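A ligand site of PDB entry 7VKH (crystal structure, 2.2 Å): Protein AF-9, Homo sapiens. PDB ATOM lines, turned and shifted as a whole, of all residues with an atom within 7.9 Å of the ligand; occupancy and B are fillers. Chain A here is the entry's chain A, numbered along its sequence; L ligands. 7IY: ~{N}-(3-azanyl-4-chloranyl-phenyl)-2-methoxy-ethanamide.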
ATOM      1  N   GLU A  26     -15.233 -32.603  -0.865  1.00  0.00           N
ATOM      2  CA  GLU A  26     -13.951 -32.086  -0.403  1.00  0.00           C
ATOM      3  C   GLU A  26     -13.598 -32.546   1.001  1.00  0.00           C
ATOM      4  O   GLU A  26     -12.501 -32.254   1.478  1.00  0.00           O
ATOM      5  CB  GLU A  26     -13.955 -30.555  -0.466  1.00  0.00           C
ATOM      6  CG  GLU A  26     -14.208 -29.977  -1.840  1.00  0.00           C
ATOM      7  CD  GLU A  26     -15.665 -29.596  -2.065  1.00  0.00           C
ATOM      8  OE1 GLU A  26     -16.511 -29.907  -1.195  1.00  0.00           O
ATOM      9  OE2 GLU A  26     -15.972 -28.984  -3.110  1.00  0.00           O
ATOM     10  N   GLY A  27     -14.503 -33.258   1.679  1.00  0.00           N
ATOM     11  CA  GLY A  27     -14.252 -33.614   3.062  1.00  0.00           C
ATOM     12  C   GLY A  27     -14.617 -32.552   4.061  1.00  0.00           C
ATOM     13  O   GLY A  27     -14.191 -32.621   5.216  1.00  0.00           O
ATOM     14  N   PHE A  28     -15.389 -31.544   3.646  1.00  0.00           N
ATOM     15  CA  PHE A  28     -15.841 -30.506   4.578  1.00  0.00           C
ATOM     16  C   PHE A  28     -16.877 -31.102   5.533  1.00  0.00           C
ATOM     17  O   PHE A  28     -17.869 -31.680   5.092  1.00  0.00           O
ATOM     18  CB  PHE A  28     -16.438 -29.325   3.821  1.00  0.00           C
ATOM     19  CG  PHE A  28     -15.483 -28.662   2.860  1.00  0.00           C
ATOM     20  CD1 PHE A  28     -14.108 -28.818   2.988  1.00  0.00           C
ATOM     21  CD2 PHE A  28     -15.967 -27.865   1.826  1.00  0.00           C
ATOM     22  CE1 PHE A  28     -13.246 -28.215   2.098  1.00  0.00           C
ATOM     23  CE2 PHE A  28     -15.110 -27.247   0.942  1.00  0.00           C
ATOM     24  CZ  PHE A  28     -13.746 -27.419   1.072  1.00  0.00           C
ATOM     25  N   THR A  29     -16.621 -30.949   6.829  1.00  0.00           N
ATOM     26  CA  THR A  29     -17.435 -31.590   7.848  1.00  0.00           C
ATOM     27  C   THR A  29     -18.549 -30.700   8.405  1.00  0.00           C
ATOM     28  O   THR A  29     -19.499 -31.223   8.994  1.00  0.00           O
ATOM     29  CB  THR A  29     -16.548 -32.060   9.005  1.00  0.00           C
ATOM     30  OG1 THR A  29     -15.910 -30.934   9.617  1.00  0.00           O
ATOM     31  CG2 THR A  29     -15.477 -33.012   8.488  1.00  0.00           C
ATOM     32  N   HIS A  30     -18.440 -29.383   8.229  1.00  0.00           N
ATOM     33  CA  HIS A  30     -19.353 -28.426   8.855  1.00  0.00           C
ATOM     34  C   HIS A  30     -19.981 -27.533   7.802  1.00  0.00           C
ATOM     35  O   HIS A  30     -19.306 -27.104   6.858  1.00  0.00           O
ATOM     36  CB  HIS A  30     -18.629 -27.535   9.867  1.00  0.00           C
ATOM     37  CG  HIS A  30     -18.243 -28.231  11.137  1.00  0.00           C
ATOM     38  ND1 HIS A  30     -17.257 -29.190  11.202  1.00  0.00           N
ATOM     39  CD2 HIS A  30     -18.684 -28.067  12.408  1.00  0.00           C
ATOM     40  CE1 HIS A  30     -17.124 -29.607  12.447  1.00  0.00           C
ATOM     41  NE2 HIS A  30     -17.975 -28.941  13.206  1.00  0.00           N
ATOM     42  N   TRP A  32     -21.608 -23.722   7.882  1.00  0.00           N
ATOM     43  CA  TRP A  32     -21.667 -22.549   8.737  1.00  0.00           C
ATOM     44  C   TRP A  32     -22.202 -21.350   7.978  1.00  0.00           C
ATOM     45  O   TRP A  32     -22.169 -21.302   6.742  1.00  0.00           O
ATOM     46  CB  TRP A  32     -20.307 -22.197   9.362  1.00  0.00           C
ATOM     47  CG  TRP A  32     -19.140 -22.043   8.420  1.00  0.00           C
ATOM     48  CD1 TRP A  32     -18.207 -22.993   8.117  1.00  0.00           C
ATOM     49  CD2 TRP A  32     -18.752 -20.859   7.707  1.00  0.00           C
ATOM     50  NE1 TRP A  32     -17.284 -22.479   7.247  1.00  0.00           N
ATOM     51  CE2 TRP A  32     -17.584 -21.176   6.981  1.00  0.00           C
ATOM     52  CE3 TRP A  32     -19.275 -19.563   7.606  1.00  0.00           C
ATOM     53  CZ2 TRP A  32     -16.936 -20.245   6.168  1.00  0.00           C
ATOM     54  CZ3 TRP A  32     -18.633 -18.640   6.794  1.00  0.00           C
ATOM     55  CH2 TRP A  32     -17.476 -18.984   6.084  1.00  0.00           C
ATOM     56  N   LEU A  55     -12.936 -14.248   3.996  1.00  0.00           N
ATOM     57  CA  LEU A  55     -12.797 -15.649   4.350  1.00  0.00           C
ATOM     58  C   LEU A  55     -11.321 -16.060   4.364  1.00  0.00           C
ATOM     59  O   LEU A  55     -10.446 -15.333   3.900  1.00  0.00           O
ATOM     60  CB  LEU A  55     -13.562 -16.543   3.372  1.00  0.00           C
ATOM     61  CG  LEU A  55     -15.016 -16.228   3.039  1.00  0.00           C
ATOM     62  CD1 LEU A  55     -15.699 -17.465   2.460  1.00  0.00           C
ATOM     63  CD2 LEU A  55     -15.782 -15.740   4.256  1.00  0.00           C
ATOM     64  N   HIS A  56     -11.069 -17.255   4.907  1.00  0.00           N
ATOM     65  CA  HIS A  56      -9.725 -17.816   4.861  1.00  0.00           C
ATOM     66  C   HIS A  56      -9.298 -18.019   3.417  1.00  0.00           C
ATOM     67  O   HIS A  56     -10.116 -18.290   2.539  1.00  0.00           O
ATOM     68  CB  HIS A  56      -9.685 -19.139   5.629  1.00  0.00           C
ATOM     69  CG  HIS A  56      -8.307 -19.690   5.822  1.00  0.00           C
ATOM     70  ND1 HIS A  56      -7.683 -20.503   4.904  1.00  0.00           N
ATOM     71  CD2 HIS A  56      -7.438 -19.555   6.848  1.00  0.00           C
ATOM     72  CE1 HIS A  56      -6.490 -20.843   5.345  1.00  0.00           C
ATOM     73  NE2 HIS A  56      -6.312 -20.275   6.520  1.00  0.00           N
ATOM     74  N   GLU A  57      -7.994 -17.871   3.182  1.00  0.00           N
ATOM     75  CA  GLU A  57      -7.448 -17.923   1.827  1.00  0.00           C
ATOM     76  C   GLU A  57      -7.728 -19.248   1.110  1.00  0.00           C
ATOM     77  O   GLU A  57      -7.673 -19.301  -0.123  1.00  0.00           O
ATOM     78  CB  GLU A  57      -5.940 -17.680   1.877  1.00  0.00           C
ATOM     79  CG  GLU A  57      -5.210 -18.724   2.699  1.00  0.00           C
ATOM     80  CD  GLU A  57      -3.827 -19.051   2.164  1.00  0.00           C
ATOM     81  OE1 GLU A  57      -2.886 -19.106   2.975  1.00  0.00           O
ATOM     82  OE2 GLU A  57      -3.705 -19.270   0.943  1.00  0.00           O
ATOM     83  N   SER A  58      -8.027 -20.304   1.859  1.00  0.00           N
ATOM     84  CA  SER A  58      -8.361 -21.581   1.223  1.00  0.00           C
ATOM     85  C   SER A  58      -9.680 -21.537   0.489  1.00  0.00           C
ATOM     86  O   SER A  58      -9.919 -22.398  -0.378  1.00  0.00           O
ATOM     87  CB  SER A  58      -8.396 -22.689   2.283  1.00  0.00           C
ATOM     88  OG  SER A  58      -9.402 -22.439   3.237  1.00  0.00           O
ATOM     89  N   PHE A  59     -10.550 -20.579   0.804  1.00  0.00           N
ATOM     90  CA  PHE A  59     -11.828 -20.485   0.107  1.00  0.00           C
ATOM     91  C   PHE A  59     -11.642 -19.790  -1.244  1.00  0.00           C
ATOM     92  O   PHE A  59     -10.830 -18.873  -1.362  1.00  0.00           O
ATOM     93  CB  PHE A  59     -12.848 -19.706   0.933  1.00  0.00           C
ATOM     94  CG  PHE A  59     -13.464 -20.507   2.045  1.00  0.00           C
ATOM     95  CD1 PHE A  59     -14.560 -21.315   1.809  1.00  0.00           C
ATOM     96  CD2 PHE A  59     -12.950 -20.447   3.332  1.00  0.00           C
ATOM     97  CE1 PHE A  59     -15.137 -22.057   2.828  1.00  0.00           C
ATOM     98  CE2 PHE A  59     -13.513 -21.186   4.352  1.00  0.00           C
ATOM     99  CZ  PHE A  59     -14.613 -21.994   4.095  1.00  0.00           C
ATOM    100  N   PRO A  60     -12.378 -20.211  -2.271  1.00  0.00           N
ATOM    101  CA  PRO A  60     -12.353 -19.479  -3.542  1.00  0.00           C
ATOM    102  C   PRO A  60     -12.995 -18.112  -3.371  1.00  0.00           C
ATOM    103  O   PRO A  60     -14.052 -17.973  -2.759  1.00  0.00           O
ATOM    104  CB  PRO A  60     -13.180 -20.361  -4.474  1.00  0.00           C
ATOM    105  CG  PRO A  60     -14.132 -21.068  -3.552  1.00  0.00           C
ATOM    106  CD  PRO A  60     -13.340 -21.325  -2.299  1.00  0.00           C
ATOM    107  N   GLU A  75     -21.465 -21.027   3.969  1.00  0.00           N
ATOM    108  CA  GLU A  75     -20.361 -21.797   3.438  1.00  0.00           C
ATOM    109  C   GLU A  75     -20.263 -23.143   4.151  1.00  0.00           C
ATOM    110  O   GLU A  75     -20.974 -23.410   5.124  1.00  0.00           O
ATOM    111  CB  GLU A  75     -19.039 -21.037   3.569  1.00  0.00           C
ATOM    112  CG  GLU A  75     -18.644 -20.263   2.317  1.00  0.00           C
ATOM    113  CD  GLU A  75     -18.348 -21.157   1.135  1.00  0.00           C
ATOM    114  OE1 GLU A  75     -18.209 -22.384   1.330  1.00  0.00           O
ATOM    115  OE2 GLU A  75     -18.262 -20.629   0.014  1.00  0.00           O
ATOM    116  N   SER A  76     -19.380 -23.990   3.645  1.00  0.00           N
ATOM    117  CA  SER A  76     -19.000 -25.234   4.286  1.00  0.00           C
ATOM    118  C   SER A  76     -17.479 -25.253   4.450  1.00  0.00           C
ATOM    119  O   SER A  76     -16.759 -24.664   3.638  1.00  0.00           O
ATOM    120  CB  SER A  76     -19.458 -26.462   3.478  1.00  0.00           C
ATOM    121  OG  SER A  76     -20.869 -26.573   3.453  1.00  0.00           O
ATOM    122  N   GLY A  77     -17.012 -25.940   5.478  1.00  0.00           N
ATOM    123  CA  GLY A  77     -15.590 -26.001   5.728  1.00  0.00           C
ATOM    124  C   GLY A  77     -15.276 -27.088   6.734  1.00  0.00           C
ATOM    125  O   GLY A  77     -16.158 -27.809   7.195  1.00  0.00           O
ATOM    126  N   TYR A  78     -13.991 -27.189   7.071  1.00  0.00           N
ATOM    127  CA  TYR A  78     -13.520 -28.183   8.021  1.00  0.00           C
ATOM    128  C   TYR A  78     -12.815 -27.593   9.226  1.00  0.00           C
ATOM    129  O   TYR A  78     -12.422 -28.348  10.119  1.00  0.00           O
ATOM    130  CB  TYR A  78     -12.593 -29.195   7.340  1.00  0.00           C
ATOM    131  CG  TYR A  78     -11.274 -28.602   6.869  1.00  0.00           C
ATOM    132  CD1 TYR A  78     -10.168 -28.571   7.713  1.00  0.00           C
ATOM    133  CD2 TYR A  78     -11.146 -28.089   5.591  1.00  0.00           C
ATOM    134  CE1 TYR A  78      -8.969 -28.035   7.295  1.00  0.00           C
ATOM    135  CE2 TYR A  78      -9.947 -27.543   5.159  1.00  0.00           C
ATOM    136  CZ  TYR A  78      -8.862 -27.520   6.012  1.00  0.00           C
ATOM    137  OH  TYR A  78      -7.679 -26.975   5.587  1.00  0.00           O
ATOM    138  N   ALA A  79     -12.637 -26.267   9.288  1.00  0.00           N
ATOM    139  CA  ALA A  79     -11.903 -25.673  10.402  1.00  0.00           C
ATOM    140  C   ALA A  79     -12.375 -24.246  10.616  1.00  0.00           C
ATOM    141  O   ALA A  79     -12.897 -23.590   9.701  1.00  0.00           O
ATOM    142  CB  ALA A  79     -10.395 -25.704  10.161  1.00  0.00           C
ATOM    143  N   GLY A  80     -12.200 -23.765  11.848  1.00  0.00           N
ATOM    144  CA  GLY A  80     -12.477 -22.386  12.153  1.00  0.00           C
ATOM    145  C   GLY A  80     -11.308 -21.485  11.843  1.00  0.00           C
ATOM    146  O   GLY A  80     -10.185 -21.925  11.582  1.00  0.00           O
ATOM    147  N   PHE A  81     -11.564 -20.180  11.897  1.00  0.00           N
ATOM    148  CA  PHE A  81     -10.543 -19.183  11.546  1.00  0.00           C
ATOM    149  C   PHE A  81     -11.031 -17.811  11.986  1.00  0.00           C
ATOM    150  O   PHE A  81     -12.195 -17.635  12.339  1.00  0.00           O
ATOM    151  CB  PHE A  81     -10.238 -19.201  10.040  1.00  0.00           C
ATOM    152  CG  PHE A  81     -11.456 -18.964   9.176  1.00  0.00           C
ATOM    153  CD1 PHE A  81     -12.285 -20.019   8.829  1.00  0.00           C
ATOM    154  CD2 PHE A  81     -11.751 -17.695   8.697  1.00  0.00           C
ATOM    155  CE1 PHE A  81     -13.405 -19.804   8.026  1.00  0.00           C
ATOM    156  CE2 PHE A  81     -12.859 -17.474   7.905  1.00  0.00           C
ATOM    157  CZ  PHE A  81     -13.696 -18.534   7.569  1.00  0.00           C
ATOM    158  N   ILE A  82     -10.120 -16.841  11.949  1.00  0.00           N
ATOM    159  CA  ILE A  82     -10.481 -15.453  12.168  1.00  0.00           C
ATOM    160  C   ILE A  82     -11.052 -14.890  10.874  1.00  0.00           C
ATOM    161  O   ILE A  82     -10.420 -14.973   9.805  1.00  0.00           O
ATOM    162  CB  ILE A  82      -9.270 -14.621  12.615  1.00  0.00           C
ATOM    163  CG1 ILE A  82      -8.456 -15.371  13.679  1.00  0.00           C
ATOM    164  CG2 ILE A  82      -9.735 -13.247  13.092  1.00  0.00           C
ATOM    165  CD1 ILE A  82      -8.997 -15.243  15.076  1.00  0.00           C
ATOM    166  N   LEU A 104     -14.744 -17.207  13.900  1.00  0.00           N
ATOM    167  CA  LEU A 104     -15.615 -18.210  13.282  1.00  0.00           C
ATOM    168  C   LEU A 104     -15.152 -19.580  13.777  1.00  0.00           C
ATOM    169  O   LEU A 104     -14.292 -20.205  13.178  1.00  0.00           O
ATOM    170  CB  LEU A 104     -15.558 -18.108  11.769  1.00  0.00           C
ATOM    171  CG  LEU A 104     -16.653 -18.681  10.865  1.00  0.00           C
ATOM    172  CD1 LEU A 104     -16.716 -20.214  10.934  1.00  0.00           C
ATOM    173  CD2 LEU A 104     -17.991 -18.059  11.194  1.00  0.00           C
ATOM    174  N   LEU A 106     -15.931 -23.615  15.133  1.00  0.00           N
ATOM    175  CA  LEU A 106     -16.794 -24.759  14.944  1.00  0.00           C
ATOM    176  C   LEU A 106     -16.646 -25.705  16.137  1.00  0.00           C
ATOM    177  O   LEU A 106     -15.563 -25.803  16.726  1.00  0.00           O
ATOM    178  CB  LEU A 106     -16.468 -25.507  13.640  1.00  0.00           C
ATOM    179  CG  LEU A 106     -16.051 -24.670  12.428  1.00  0.00           C
ATOM    180  CD1 LEU A 106     -15.469 -25.573  11.357  1.00  0.00           C
ATOM    181  CD2 LEU A 106     -17.220 -23.884  11.881  1.00  0.00           C
HETATM  182  C14 7IY L   1     -11.596 -24.672   1.485  1.00  0.00           C
HETATM  183  C5  7IY L   1      -9.855 -23.599   6.151  1.00  0.00           C
HETATM  184  C6  7IY L   1      -8.409 -22.789   8.369  1.00  0.00           C
HETATM  185  C8  7IY L   1      -9.762 -22.508   8.284  1.00  0.00           C
HETATM  186  C10 7IY L   1     -10.488 -22.912   7.168  1.00  0.00           C
HETATM  187  C12 7IY L   1     -12.478 -25.073   3.625  1.00  0.00           C
HETATM  188  C3  7IY L   1     -11.873 -24.653   4.964  1.00  0.00           C
HETATM  189  C1  7IY L   1      -7.774 -23.478   7.343  1.00  0.00           C
HETATM  190  C2  7IY L   1      -8.502 -23.879   6.237  1.00  0.00           C
HETATM  191  N4  7IY L   1     -10.559 -24.041   4.956  1.00  0.00           N
HETATM  192  N9  7IY L   1      -6.355 -23.781   7.418  1.00  0.00           N
HETATM  193  O13 7IY L   1     -12.097 -24.128   2.661  1.00  0.00           O
HETATM  194  O7  7IY L   1     -12.477 -24.830   5.967  1.00  0.00           O
HETATM  195 CL1  7IY L   1      -7.462 -22.285   9.795  1.00  0.00          CL
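The side-chain hydroxyl (OG) of Ser 58 is in hydrogen-bond range of a nitrogen (N4) of the ligand, at 2.6 Å. N of Tyr 78 lies within hydrogen-bond range of O7 of the ligand (3.0 Å).
A ring nitrogen (ND1) of His 56 lies close to the backbone NH of Ser 58 (3.1 Å). The backbone NH (N) of Thr 29 is in hydrogen-bond range of the backbone carbonyl oxygen (O) of Gly 77. The backbone NH (N) of Gly 77 is in hydrogen-bond range of the backbone carbonyl oxygen (O) of His 30. N of Phe 81 lies within hydrogen-bond range of O of Leu 104, at 3.0 Å.
Merely in contact with the ligand: Gly 80 (3.3 Å), Gly 77 (3.3 Å), Phe 28 (3.5 Å), His 56 (3.5 Å), Ala 79 (3.6 Å), Phe 81 (3.6 Å) and Phe 59 (3.6 Å). Hydrophobic or aromatic side chains within 4 Å of the ligand: Phe 28, His 56, Phe 59, Tyr 78, Ala 79 and Phe 81. Of the 22 residues printed, 9 come within 4 Å of the ligand.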
